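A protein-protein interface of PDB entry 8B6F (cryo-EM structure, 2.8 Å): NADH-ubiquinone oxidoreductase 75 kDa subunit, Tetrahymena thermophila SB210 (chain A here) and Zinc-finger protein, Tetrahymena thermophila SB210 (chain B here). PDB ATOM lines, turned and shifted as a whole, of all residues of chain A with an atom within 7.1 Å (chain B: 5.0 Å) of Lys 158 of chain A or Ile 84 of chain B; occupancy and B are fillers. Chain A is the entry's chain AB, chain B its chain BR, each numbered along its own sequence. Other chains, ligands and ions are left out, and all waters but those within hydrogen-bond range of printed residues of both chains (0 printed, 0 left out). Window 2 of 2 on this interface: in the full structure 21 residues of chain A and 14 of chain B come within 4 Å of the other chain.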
ATOM      1  N   LEU A 122      23.737  -0.244  -9.106  1.00  0.00           N
ATOM      2  CA  LEU A 122      23.139  -0.485  -7.800  1.00  0.00           C
ATOM      3  C   LEU A 122      22.002  -1.490  -7.872  1.00  0.00           C
ATOM      4  O   LEU A 122      21.700  -2.138  -6.865  1.00  0.00           O
ATOM      5  CB  LEU A 122      22.654   0.830  -7.193  1.00  0.00           C
ATOM      6  CG  LEU A 122      23.768   1.834  -6.881  1.00  0.00           C
ATOM      7  CD1 LEU A 122      23.181   3.127  -6.367  1.00  0.00           C
ATOM      8  CD2 LEU A 122      24.767   1.275  -5.877  1.00  0.00           C
ATOM      9  N   ALA A 123      21.364  -1.632  -9.028  1.00  0.00           N
ATOM     10  CA  ALA A 123      20.374  -2.683  -9.199  1.00  0.00           C
ATOM     11  C   ALA A 123      21.043  -4.029  -8.957  1.00  0.00           C
ATOM     12  O   ALA A 123      22.127  -4.299  -9.482  1.00  0.00           O
ATOM     13  CB  ALA A 123      19.761  -2.628 -10.598  1.00  0.00           C
ATOM     14  N   ASN A 124      20.397  -4.870  -8.160  1.00  0.00           N
ATOM     15  CA  ASN A 124      20.872  -6.179  -7.732  1.00  0.00           C
ATOM     16  C   ASN A 124      21.965  -6.074  -6.663  1.00  0.00           C
ATOM     17  O   ASN A 124      22.425  -7.116  -6.184  1.00  0.00           O
ATOM     18  CB  ASN A 124      21.389  -7.023  -8.909  1.00  0.00           C
ATOM     19  CG  ASN A 124      20.356  -7.173 -10.013  1.00  0.00           C
ATOM     20  OD1 ASN A 124      20.336  -6.393 -10.961  1.00  0.00           O
ATOM     21  ND2 ASN A 124      19.494  -8.176  -9.896  1.00  0.00           N
ATOM     22  N   HIS A 125      22.394  -4.866  -6.268  1.00  0.00           N
ATOM     23  CA  HIS A 125      23.455  -4.727  -5.268  1.00  0.00           C
ATOM     24  C   HIS A 125      22.883  -4.945  -3.873  1.00  0.00           C
ATOM     25  O   HIS A 125      21.898  -4.296  -3.507  1.00  0.00           O
ATOM     26  CB  HIS A 125      24.114  -3.346  -5.309  1.00  0.00           C
ATOM     27  CG  HIS A 125      25.502  -3.314  -4.731  1.00  0.00           C
ATOM     28  ND1 HIS A 125      26.474  -4.244  -5.032  1.00  0.00           N
ATOM     29  CD2 HIS A 125      26.052  -2.484  -3.810  1.00  0.00           C
ATOM     30  CE1 HIS A 125      27.575  -3.961  -4.355  1.00  0.00           C
ATOM     31  NE2 HIS A 125      27.343  -2.907  -3.593  1.00  0.00           N
ATOM     32  N   PRO A 126      23.467  -5.832  -3.071  1.00  0.00           N
ATOM     33  CA  PRO A 126      22.872  -6.146  -1.770  1.00  0.00           C
ATOM     34  C   PRO A 126      22.959  -4.965  -0.821  1.00  0.00           C
ATOM     35  O   PRO A 126      23.837  -4.108  -0.933  1.00  0.00           O
ATOM     36  CB  PRO A 126      23.714  -7.322  -1.273  1.00  0.00           C
ATOM     37  CG  PRO A 126      25.035  -7.112  -1.909  1.00  0.00           C
ATOM     38  CD  PRO A 126      24.747  -6.535  -3.266  1.00  0.00           C
ATOM     39  N   LEU A 127      22.027  -4.931   0.126  1.00  0.00           N
ATOM     40  CA  LEU A 127      22.005  -3.885   1.146  1.00  0.00           C
ATOM     41  C   LEU A 127      22.892  -4.308   2.319  1.00  0.00           C
ATOM     42  O   LEU A 127      22.427  -4.661   3.403  1.00  0.00           O
ATOM     43  CB  LEU A 127      20.569  -3.630   1.591  1.00  0.00           C
ATOM     44  CG  LEU A 127      19.528  -3.394   0.492  1.00  0.00           C
ATOM     45  CD1 LEU A 127      18.222  -2.898   1.089  1.00  0.00           C
ATOM     46  CD2 LEU A 127      20.036  -2.411  -0.535  1.00  0.00           C
ATOM     47  N   SER A 152      16.378   4.988  -5.748  1.00  0.00           N
ATOM     48  CA  SER A 152      16.369   3.861  -6.666  1.00  0.00           C
ATOM     49  C   SER A 152      14.937   3.467  -7.005  1.00  0.00           C
ATOM     50  O   SER A 152      14.019   3.644  -6.200  1.00  0.00           O
ATOM     51  CB  SER A 152      17.106   2.662  -6.062  1.00  0.00           C
ATOM     52  OG  SER A 152      17.180   1.586  -6.982  1.00  0.00           O
ATOM     53  N   TYR A 154      14.455   0.216  -8.708  1.00  0.00           N
ATOM     54  CA  TYR A 154      14.421  -1.237  -8.788  1.00  0.00           C
ATOM     55  C   TYR A 154      13.803  -1.818  -7.526  1.00  0.00           C
ATOM     56  O   TYR A 154      14.425  -1.802  -6.460  1.00  0.00           O
ATOM     57  CB  TYR A 154      15.832  -1.786  -8.998  1.00  0.00           C
ATOM     58  CG  TYR A 154      15.895  -3.277  -9.224  1.00  0.00           C
ATOM     59  CD1 TYR A 154      15.967  -4.161  -8.156  1.00  0.00           C
ATOM     60  CD2 TYR A 154      15.901  -3.801 -10.510  1.00  0.00           C
ATOM     61  CE1 TYR A 154      16.031  -5.525  -8.361  1.00  0.00           C
ATOM     62  CE2 TYR A 154      15.966  -5.163 -10.725  1.00  0.00           C
ATOM     63  CZ  TYR A 154      16.033  -6.020  -9.647  1.00  0.00           C
ATOM     64  OH  TYR A 154      16.097  -7.377  -9.858  1.00  0.00           O
ATOM     65  N   ASN A 155      12.581  -2.331  -7.636  1.00  0.00           N
ATOM     66  CA  ASN A 155      11.881  -2.976  -6.527  1.00  0.00           C
ATOM     67  C   ASN A 155      11.538  -4.390  -6.978  1.00  0.00           C
ATOM     68  O   ASN A 155      10.418  -4.666  -7.412  1.00  0.00           O
ATOM     69  CB  ASN A 155      10.630  -2.171  -6.135  1.00  0.00           C
ATOM     70  CG  ASN A 155       9.813  -2.848  -5.056  1.00  0.00           C
ATOM     71  OD1 ASN A 155       8.927  -3.649  -5.347  1.00  0.00           O
ATOM     72  ND2 ASN A 155      10.103  -2.525  -3.801  1.00  0.00           N
ATOM     73  N   GLU A 156      12.506  -5.292  -6.843  1.00  0.00           N
ATOM     74  CA  GLU A 156      12.378  -6.665  -7.308  1.00  0.00           C
ATOM     75  C   GLU A 156      13.430  -7.503  -6.598  1.00  0.00           C
ATOM     76  O   GLU A 156      14.328  -6.978  -5.936  1.00  0.00           O
ATOM     77  CB  GLU A 156      12.550  -6.768  -8.829  1.00  0.00           C
ATOM     78  CG  GLU A 156      11.502  -6.036  -9.647  1.00  0.00           C
ATOM     79  CD  GLU A 156      11.740  -6.166 -11.130  1.00  0.00           C
ATOM     80  OE1 GLU A 156      12.861  -6.553 -11.517  1.00  0.00           O
ATOM     81  OE2 GLU A 156      10.808  -5.878 -11.910  1.00  0.00           O
ATOM     82  N   TYR A 157      13.310  -8.819  -6.746  1.00  0.00           N
ATOM     83  CA  TYR A 157      14.319  -9.719  -6.204  1.00  0.00           C
ATOM     84  C   TYR A 157      15.669  -9.449  -6.854  1.00  0.00           C
ATOM     85  O   TYR A 157      15.771  -9.324  -8.077  1.00  0.00           O
ATOM     86  CB  TYR A 157      13.904 -11.173  -6.422  1.00  0.00           C
ATOM     87  CG  TYR A 157      13.083 -11.741  -5.292  1.00  0.00           C
ATOM     88  CD1 TYR A 157      11.818 -11.245  -5.008  1.00  0.00           C
ATOM     89  CD2 TYR A 157      13.568 -12.782  -4.514  1.00  0.00           C
ATOM     90  CE1 TYR A 157      11.064 -11.764  -3.976  1.00  0.00           C
ATOM     91  CE2 TYR A 157      12.821 -13.307  -3.480  1.00  0.00           C
ATOM     92  CZ  TYR A 157      11.570 -12.795  -3.217  1.00  0.00           C
ATOM     93  OH  TYR A 157      10.823 -13.318  -2.188  1.00  0.00           O
ATOM     94  N   LYS A 158      16.706  -9.359  -6.029  1.00  0.00           N
ATOM     95  CA  LYS A 158      18.052  -9.093  -6.502  1.00  0.00           C
ATOM     96  C   LYS A 158      18.776 -10.398  -6.824  1.00  0.00           C
ATOM     97  O   LYS A 158      18.313 -11.494  -6.506  1.00  0.00           O
ATOM     98  CB  LYS A 158      18.839  -8.300  -5.459  1.00  0.00           C
ATOM     99  CG  LYS A 158      18.279  -6.918  -5.168  1.00  0.00           C
ATOM    100  CD  LYS A 158      19.115  -6.206  -4.118  1.00  0.00           C
ATOM    101  CE  LYS A 158      18.660  -4.772  -3.913  1.00  0.00           C
ATOM    102  NZ  LYS A 158      18.889  -3.925  -5.114  1.00  0.00           N
ATOM    103  N   ARG A 159      19.926 -10.265  -7.477  1.00  0.00           N
ATOM    104  CA  ARG A 159      20.784 -11.412  -7.720  1.00  0.00           C
ATOM    105  C   ARG A 159      21.389 -11.897  -6.410  1.00  0.00           C
ATOM    106  O   ARG A 159      21.695 -11.103  -5.516  1.00  0.00           O
ATOM    107  CB  ARG A 159      21.890 -11.048  -8.711  1.00  0.00           C
ATOM    108  CG  ARG A 159      22.901 -12.161  -8.948  1.00  0.00           C
ATOM    109  CD  ARG A 159      23.972 -11.751  -9.945  1.00  0.00           C
ATOM    110  NE  ARG A 159      24.722 -10.577  -9.506  1.00  0.00           N
ATOM    111  CZ  ARG A 159      24.464  -9.329  -9.875  1.00  0.00           C
ATOM    112  NH1 ARG A 159      23.473  -9.039 -10.702  1.00  0.00           N
ATOM    113  NH2 ARG A 159      25.221  -8.343  -9.402  1.00  0.00           N
ATOM    114  N   ALA A 160      21.558 -13.211  -6.294  1.00  0.00           N
ATOM    115  CA  ALA A 160      22.183 -13.819  -5.131  1.00  0.00           C
ATOM    116  C   ALA A 160      23.251 -14.788  -5.609  1.00  0.00           C
ATOM    117  O   ALA A 160      22.981 -15.645  -6.455  1.00  0.00           O
ATOM    118  CB  ALA A 160      21.149 -14.538  -4.260  1.00  0.00           C
ATOM    119  N   VAL A 161      24.458 -14.653  -5.066  1.00  0.00           N
ATOM    120  CA  VAL A 161      25.605 -15.455  -5.471  1.00  0.00           C
ATOM    121  C   VAL A 161      26.195 -16.122  -4.240  1.00  0.00           C
ATOM    122  O   VAL A 161      26.334 -15.491  -3.186  1.00  0.00           O
ATOM    123  CB  VAL A 161      26.673 -14.602  -6.188  1.00  0.00           C
ATOM    124  CG1 VAL A 161      27.838 -15.472  -6.639  1.00  0.00           C
ATOM    125  CG2 VAL A 161      26.064 -13.867  -7.370  1.00  0.00           C
ATOM    126  N   LYS A 203      23.524 -12.211 -16.415  1.00  0.00           N
ATOM    127  CA  LYS A 203      23.502 -11.785 -15.022  1.00  0.00           C
ATOM    128  C   LYS A 203      23.949 -12.893 -14.079  1.00  0.00           C
ATOM    129  O   LYS A 203      24.259 -12.617 -12.916  1.00  0.00           O
ATOM    130  CB  LYS A 203      22.097 -11.310 -14.647  1.00  0.00           C
ATOM    131  CG  LYS A 203      22.010 -10.657 -13.278  1.00  0.00           C
ATOM    132  CD  LYS A 203      20.616 -10.117 -12.997  1.00  0.00           C
ATOM    133  CE  LYS A 203      19.599 -11.240 -12.858  1.00  0.00           C
ATOM    134  NZ  LYS A 203      18.276 -10.734 -12.391  1.00  0.00           N
ATOM    135  N   SER B  82      12.235 -22.245  -2.921  1.00  0.00           N
ATOM    136  CA  SER B  82      12.878 -21.469  -3.971  1.00  0.00           C
ATOM    137  C   SER B  82      14.398 -21.542  -3.857  1.00  0.00           C
ATOM    138  O   SER B  82      14.958 -21.875  -2.809  1.00  0.00           O
ATOM    139  CB  SER B  82      12.422 -20.012  -3.914  1.00  0.00           C
ATOM    140  OG  SER B  82      12.718 -19.433  -2.654  1.00  0.00           O
ATOM    141  N   ASN B  83      15.069 -21.232  -4.968  1.00  0.00           N
ATOM    142  CA  ASN B  83      16.526 -21.198  -4.973  1.00  0.00           C
ATOM    143  C   ASN B  83      17.066 -19.960  -4.270  1.00  0.00           C
ATOM    144  O   ASN B  83      18.201 -19.975  -3.783  1.00  0.00           O
ATOM    145  CB  ASN B  83      17.055 -21.245  -6.408  1.00  0.00           C
ATOM    146  CG  ASN B  83      16.789 -22.572  -7.084  1.00  0.00           C
ATOM    147  OD1 ASN B  83      16.728 -23.613  -6.432  1.00  0.00           O
ATOM    148  ND2 ASN B  83      16.639 -22.544  -8.403  1.00  0.00           N
ATOM    149  N   ILE B  84      16.281 -18.890  -4.216  1.00  0.00           N
ATOM    150  CA  ILE B  84      16.683 -17.630  -3.605  1.00  0.00           C
ATOM    151  C   ILE B  84      15.643 -17.269  -2.556  1.00  0.00           C
ATOM    152  O   ILE B  84      14.438 -17.346  -2.820  1.00  0.00           O
ATOM    153  CB  ILE B  84      16.825 -16.514  -4.659  1.00  0.00           C
ATOM    154  CG1 ILE B  84      17.311 -15.218  -4.006  1.00  0.00           C
ATOM    155  CG2 ILE B  84      15.502 -16.302  -5.392  1.00  0.00           C
ATOM    156  CD1 ILE B  84      17.553 -14.089  -4.990  1.00  0.00           C
ATOM    157  N   VAL B  85      16.104 -16.893  -1.366  1.00  0.00           N
ATOM    158  CA  VAL B  85      15.228 -16.588  -0.243  1.00  0.00           C
ATOM    159  C   VAL B  85      15.461 -15.146   0.182  1.00  0.00           C
ATOM    160  O   VAL B  85      16.604 -14.688   0.270  1.00  0.00           O
ATOM    161  CB  VAL B  85      15.456 -17.554   0.938  1.00  0.00           C
ATOM    162  CG1 VAL B  85      16.888 -17.476   1.435  1.00  0.00           C
ATOM    163  CG2 VAL B  85      14.477 -17.256   2.067  1.00  0.00           C
ATOM    164  N   ARG B  86      14.368 -14.436   0.440  1.00  0.00           N
ATOM    165  CA  ARG B  86      14.403 -13.047   0.876  1.00  0.00           C
ATOM    166  C   ARG B  86      14.201 -12.996   2.384  1.00  0.00           C
ATOM    167  O   ARG B  86      13.277 -13.624   2.911  1.00  0.00           O
ATOM    168  CB  ARG B  86      13.327 -12.228   0.166  1.00  0.00           C
ATOM    169  CG  ARG B  86      13.320 -10.751   0.526  1.00  0.00           C
ATOM    170  CD  ARG B  86      12.087 -10.065  -0.036  1.00  0.00           C
ATOM    171  NE  ARG B  86      10.862 -10.541   0.595  1.00  0.00           N
ATOM    172  CZ  ARG B  86       9.639 -10.217   0.197  1.00  0.00           C
ATOM    173  NH1 ARG B  86       9.437  -9.431  -0.847  1.00  0.00           N
ATOM    174  NH2 ARG B  86       8.593 -10.699   0.860  1.00  0.00           N
ATOM    175  N   TYR B 101      18.920 -10.876   0.204  1.00  0.00           N
ATOM    176  CA  TYR B 101      18.628 -12.082  -0.555  1.00  0.00           C
ATOM    177  C   TYR B 101      19.773 -13.073  -0.403  1.00  0.00           C
ATOM    178  O   TYR B 101      20.947 -12.694  -0.468  1.00  0.00           O
ATOM    179  CB  TYR B 101      18.404 -11.757  -2.033  1.00  0.00           C
ATOM    180  CG  TYR B 101      17.297 -10.758  -2.257  1.00  0.00           C
ATOM    181  CD1 TYR B 101      15.980 -11.171  -2.397  1.00  0.00           C
ATOM    182  CD2 TYR B 101      17.566  -9.399  -2.313  1.00  0.00           C
ATOM    183  CE1 TYR B 101      14.964 -10.260  -2.596  1.00  0.00           C
ATOM    184  CE2 TYR B 101      16.558  -8.479  -2.510  1.00  0.00           C
ATOM    185  CZ  TYR B 101      15.260  -8.915  -2.652  1.00  0.00           C
ATOM    186  OH  TYR B 101      14.252  -8.003  -2.850  1.00  0.00           O
ATOM    187  N   ILE B 102      19.424 -14.341  -0.204  1.00  0.00           N
ATOM    188  CA  ILE B 102      20.386 -15.409   0.039  1.00  0.00           C
ATOM    189  C   ILE B 102      20.187 -16.485  -1.018  1.00  0.00           C
ATOM    190  O   ILE B 102      19.057 -16.922  -1.261  1.00  0.00           O
ATOM    191  CB  ILE B 102      20.230 -15.997   1.454  1.00  0.00           C
ATOM    192  CG1 ILE B 102      20.448 -14.906   2.505  1.00  0.00           C
ATOM    193  CG2 ILE B 102      21.206 -17.148   1.669  1.00  0.00           C
ATOM    194  CD1 ILE B 102      20.069 -15.319   3.907  1.00  0.00           C
ATOM    195  N   GLN B 103      21.285 -16.911  -1.637  1.00  0.00           N
ATOM    196  CA  GLN B 103      21.242 -17.933  -2.676  1.00  0.00           C
ATOM    197  C   GLN B 103      21.264 -19.314  -2.034  1.00  0.00           C
ATOM    198  O   GLN B 103      22.254 -19.692  -1.399  1.00  0.00           O
ATOM    199  CB  GLN B 103      22.421 -17.772  -3.631  1.00  0.00           C
ATOM    200  CG  GLN B 103      22.442 -18.783  -4.766  1.00  0.00           C
ATOM    201  CD  GLN B 103      21.208 -18.701  -5.638  1.00  0.00           C
ATOM    202  OE1 GLN B 103      20.338 -19.568  -5.584  1.00  0.00           O
ATOM    203  NE2 GLN B 103      21.125 -17.653  -6.450  1.00  0.00           N
ATOM    204  N   LEU B 104      20.179 -20.064  -2.203  1.00  0.00           N
ATOM    205  CA  LEU B 104      20.090 -21.429  -1.701  1.00  0.00           C
ATOM    206  C   LEU B 104      20.506 -22.467  -2.734  1.00  0.00           C
ATOM    207  O   LEU B 104      20.505 -23.662  -2.425  1.00  0.00           O
ATOM    208  CB  LEU B 104      18.662 -21.722  -1.231  1.00  0.00           C
ATOM    209  CG  LEU B 104      18.070 -20.725  -0.231  1.00  0.00           C
ATOM    210  CD1 LEU B 104      16.694 -21.180   0.213  1.00  0.00           C
ATOM    211  CD2 LEU B 104      18.982 -20.536   0.968  1.00  0.00           C
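The side-chain amide nitrogen of Gln 103 of chain B lies within hydrogen-bond range of the backbone carbonyl oxygen of Ala 160 of chain A (2.7 Å).
The backbone carbonyl oxygen (O) of Glu 156 of chain A sits at hydrogen-bond distance from the side-chain hydroxyl (OH) of Tyr 101 of chain B (3.3 Å).
The side-chain amino group (NZ) of Lys 158 of chain A lies close to the backbone carbonyl oxygen (O) of His 125 of chain A (3.4 Å).
OH of Tyr 154 of chain A is in hydrogen-bond range of O of Tyr 157 of chain A (2.7 Å).
O of Asn 83 of chain B sits close to OE1 of Gln 103 of chain B, 2.8 Å away.
The backbone NH (N) of Ile 102 of chain B sits at hydrogen-bond distance from the backbone carbonyl oxygen (O) of Val 85 of chain B (2.9 Å).
The side-chain hydroxyl (OG) of Ser 82 of chain B sits at hydrogen-bond distance from the backbone carbonyl oxygen (O) of Ile 84 of chain B (2.7 Å).
CB of Arg 86 of chain B touches OH of Tyr 157 of chain A (3.6 Å).
Tyr 101 of chain B touches Tyr 157 of chain A.
Lys 158 of chain A touches Ile 84 of chain B (O to CD1, 3.1 Å).
Lys 158 of chain A touches Tyr 101 of chain B.
CB of Ala 160 of chain A touches CD1 of Ile 84 of chain B (3.7 Å).
CB of Ala 160 of chain A touches C of Ile 102 of chain B, 3.9 Å away.
Val 161 of chain A touches Gln 103 of chain B (N to CB, 3.99 Å).
Of the printed residues of chain B, Tyr 157 of chain A touches Arg 86 (3.6 Å) and Tyr 101 (3.5 Å).
Lys 158 of chain A touches just these residues of chain B: Ile 84 (3.1 Å) and Tyr 101 (3.5 Å).
Printed residues of chain B within 4 Å of Ala 160 of chain A: Ile 84 (3.7 Å), Ile 102 (3.9 Å) and Gln 103 (2.7 Å).
Of the printed residues of chain B, Val 161 of chain A touches Gln 103.
Ile 84 of chain B touches just these residues of chain A: Lys 158 and Ala 160.
Printed residues of chain A within 4 Å of Arg 86 of chain B: Tyr 157.
Printed residues of chain A within 4 Å of Ile 102 of chain B: Ala 160 (3.9 Å).
The nearest printed residue of chain B that does not touch Lys 158 of chain A is Gln 103 of chain B (6.8 Å).
Of the 9 printed residues of chain B, 5 touch a printed residue of chain A.
Hydrophobic or aromatic side chains of chain B that line the printed part of chain A: Ile 84 and Tyr 101.
Along chain B the printed residues that touch a printed residue of chain A span positions 84 to 103.
Of the 16 printed residues of chain A, 5 touch a printed residue of chain B.
Hydrophobic or aromatic side chains of chain A that line the printed part of chain B: Tyr 157 and Ala 160.
Among the printed residues, 9 pairs touch across the chains.
Among the printed residues, no Asp or Glu carboxylate lies within 4 Å of a Lys or Arg side-chain nitrogen of the other chain.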
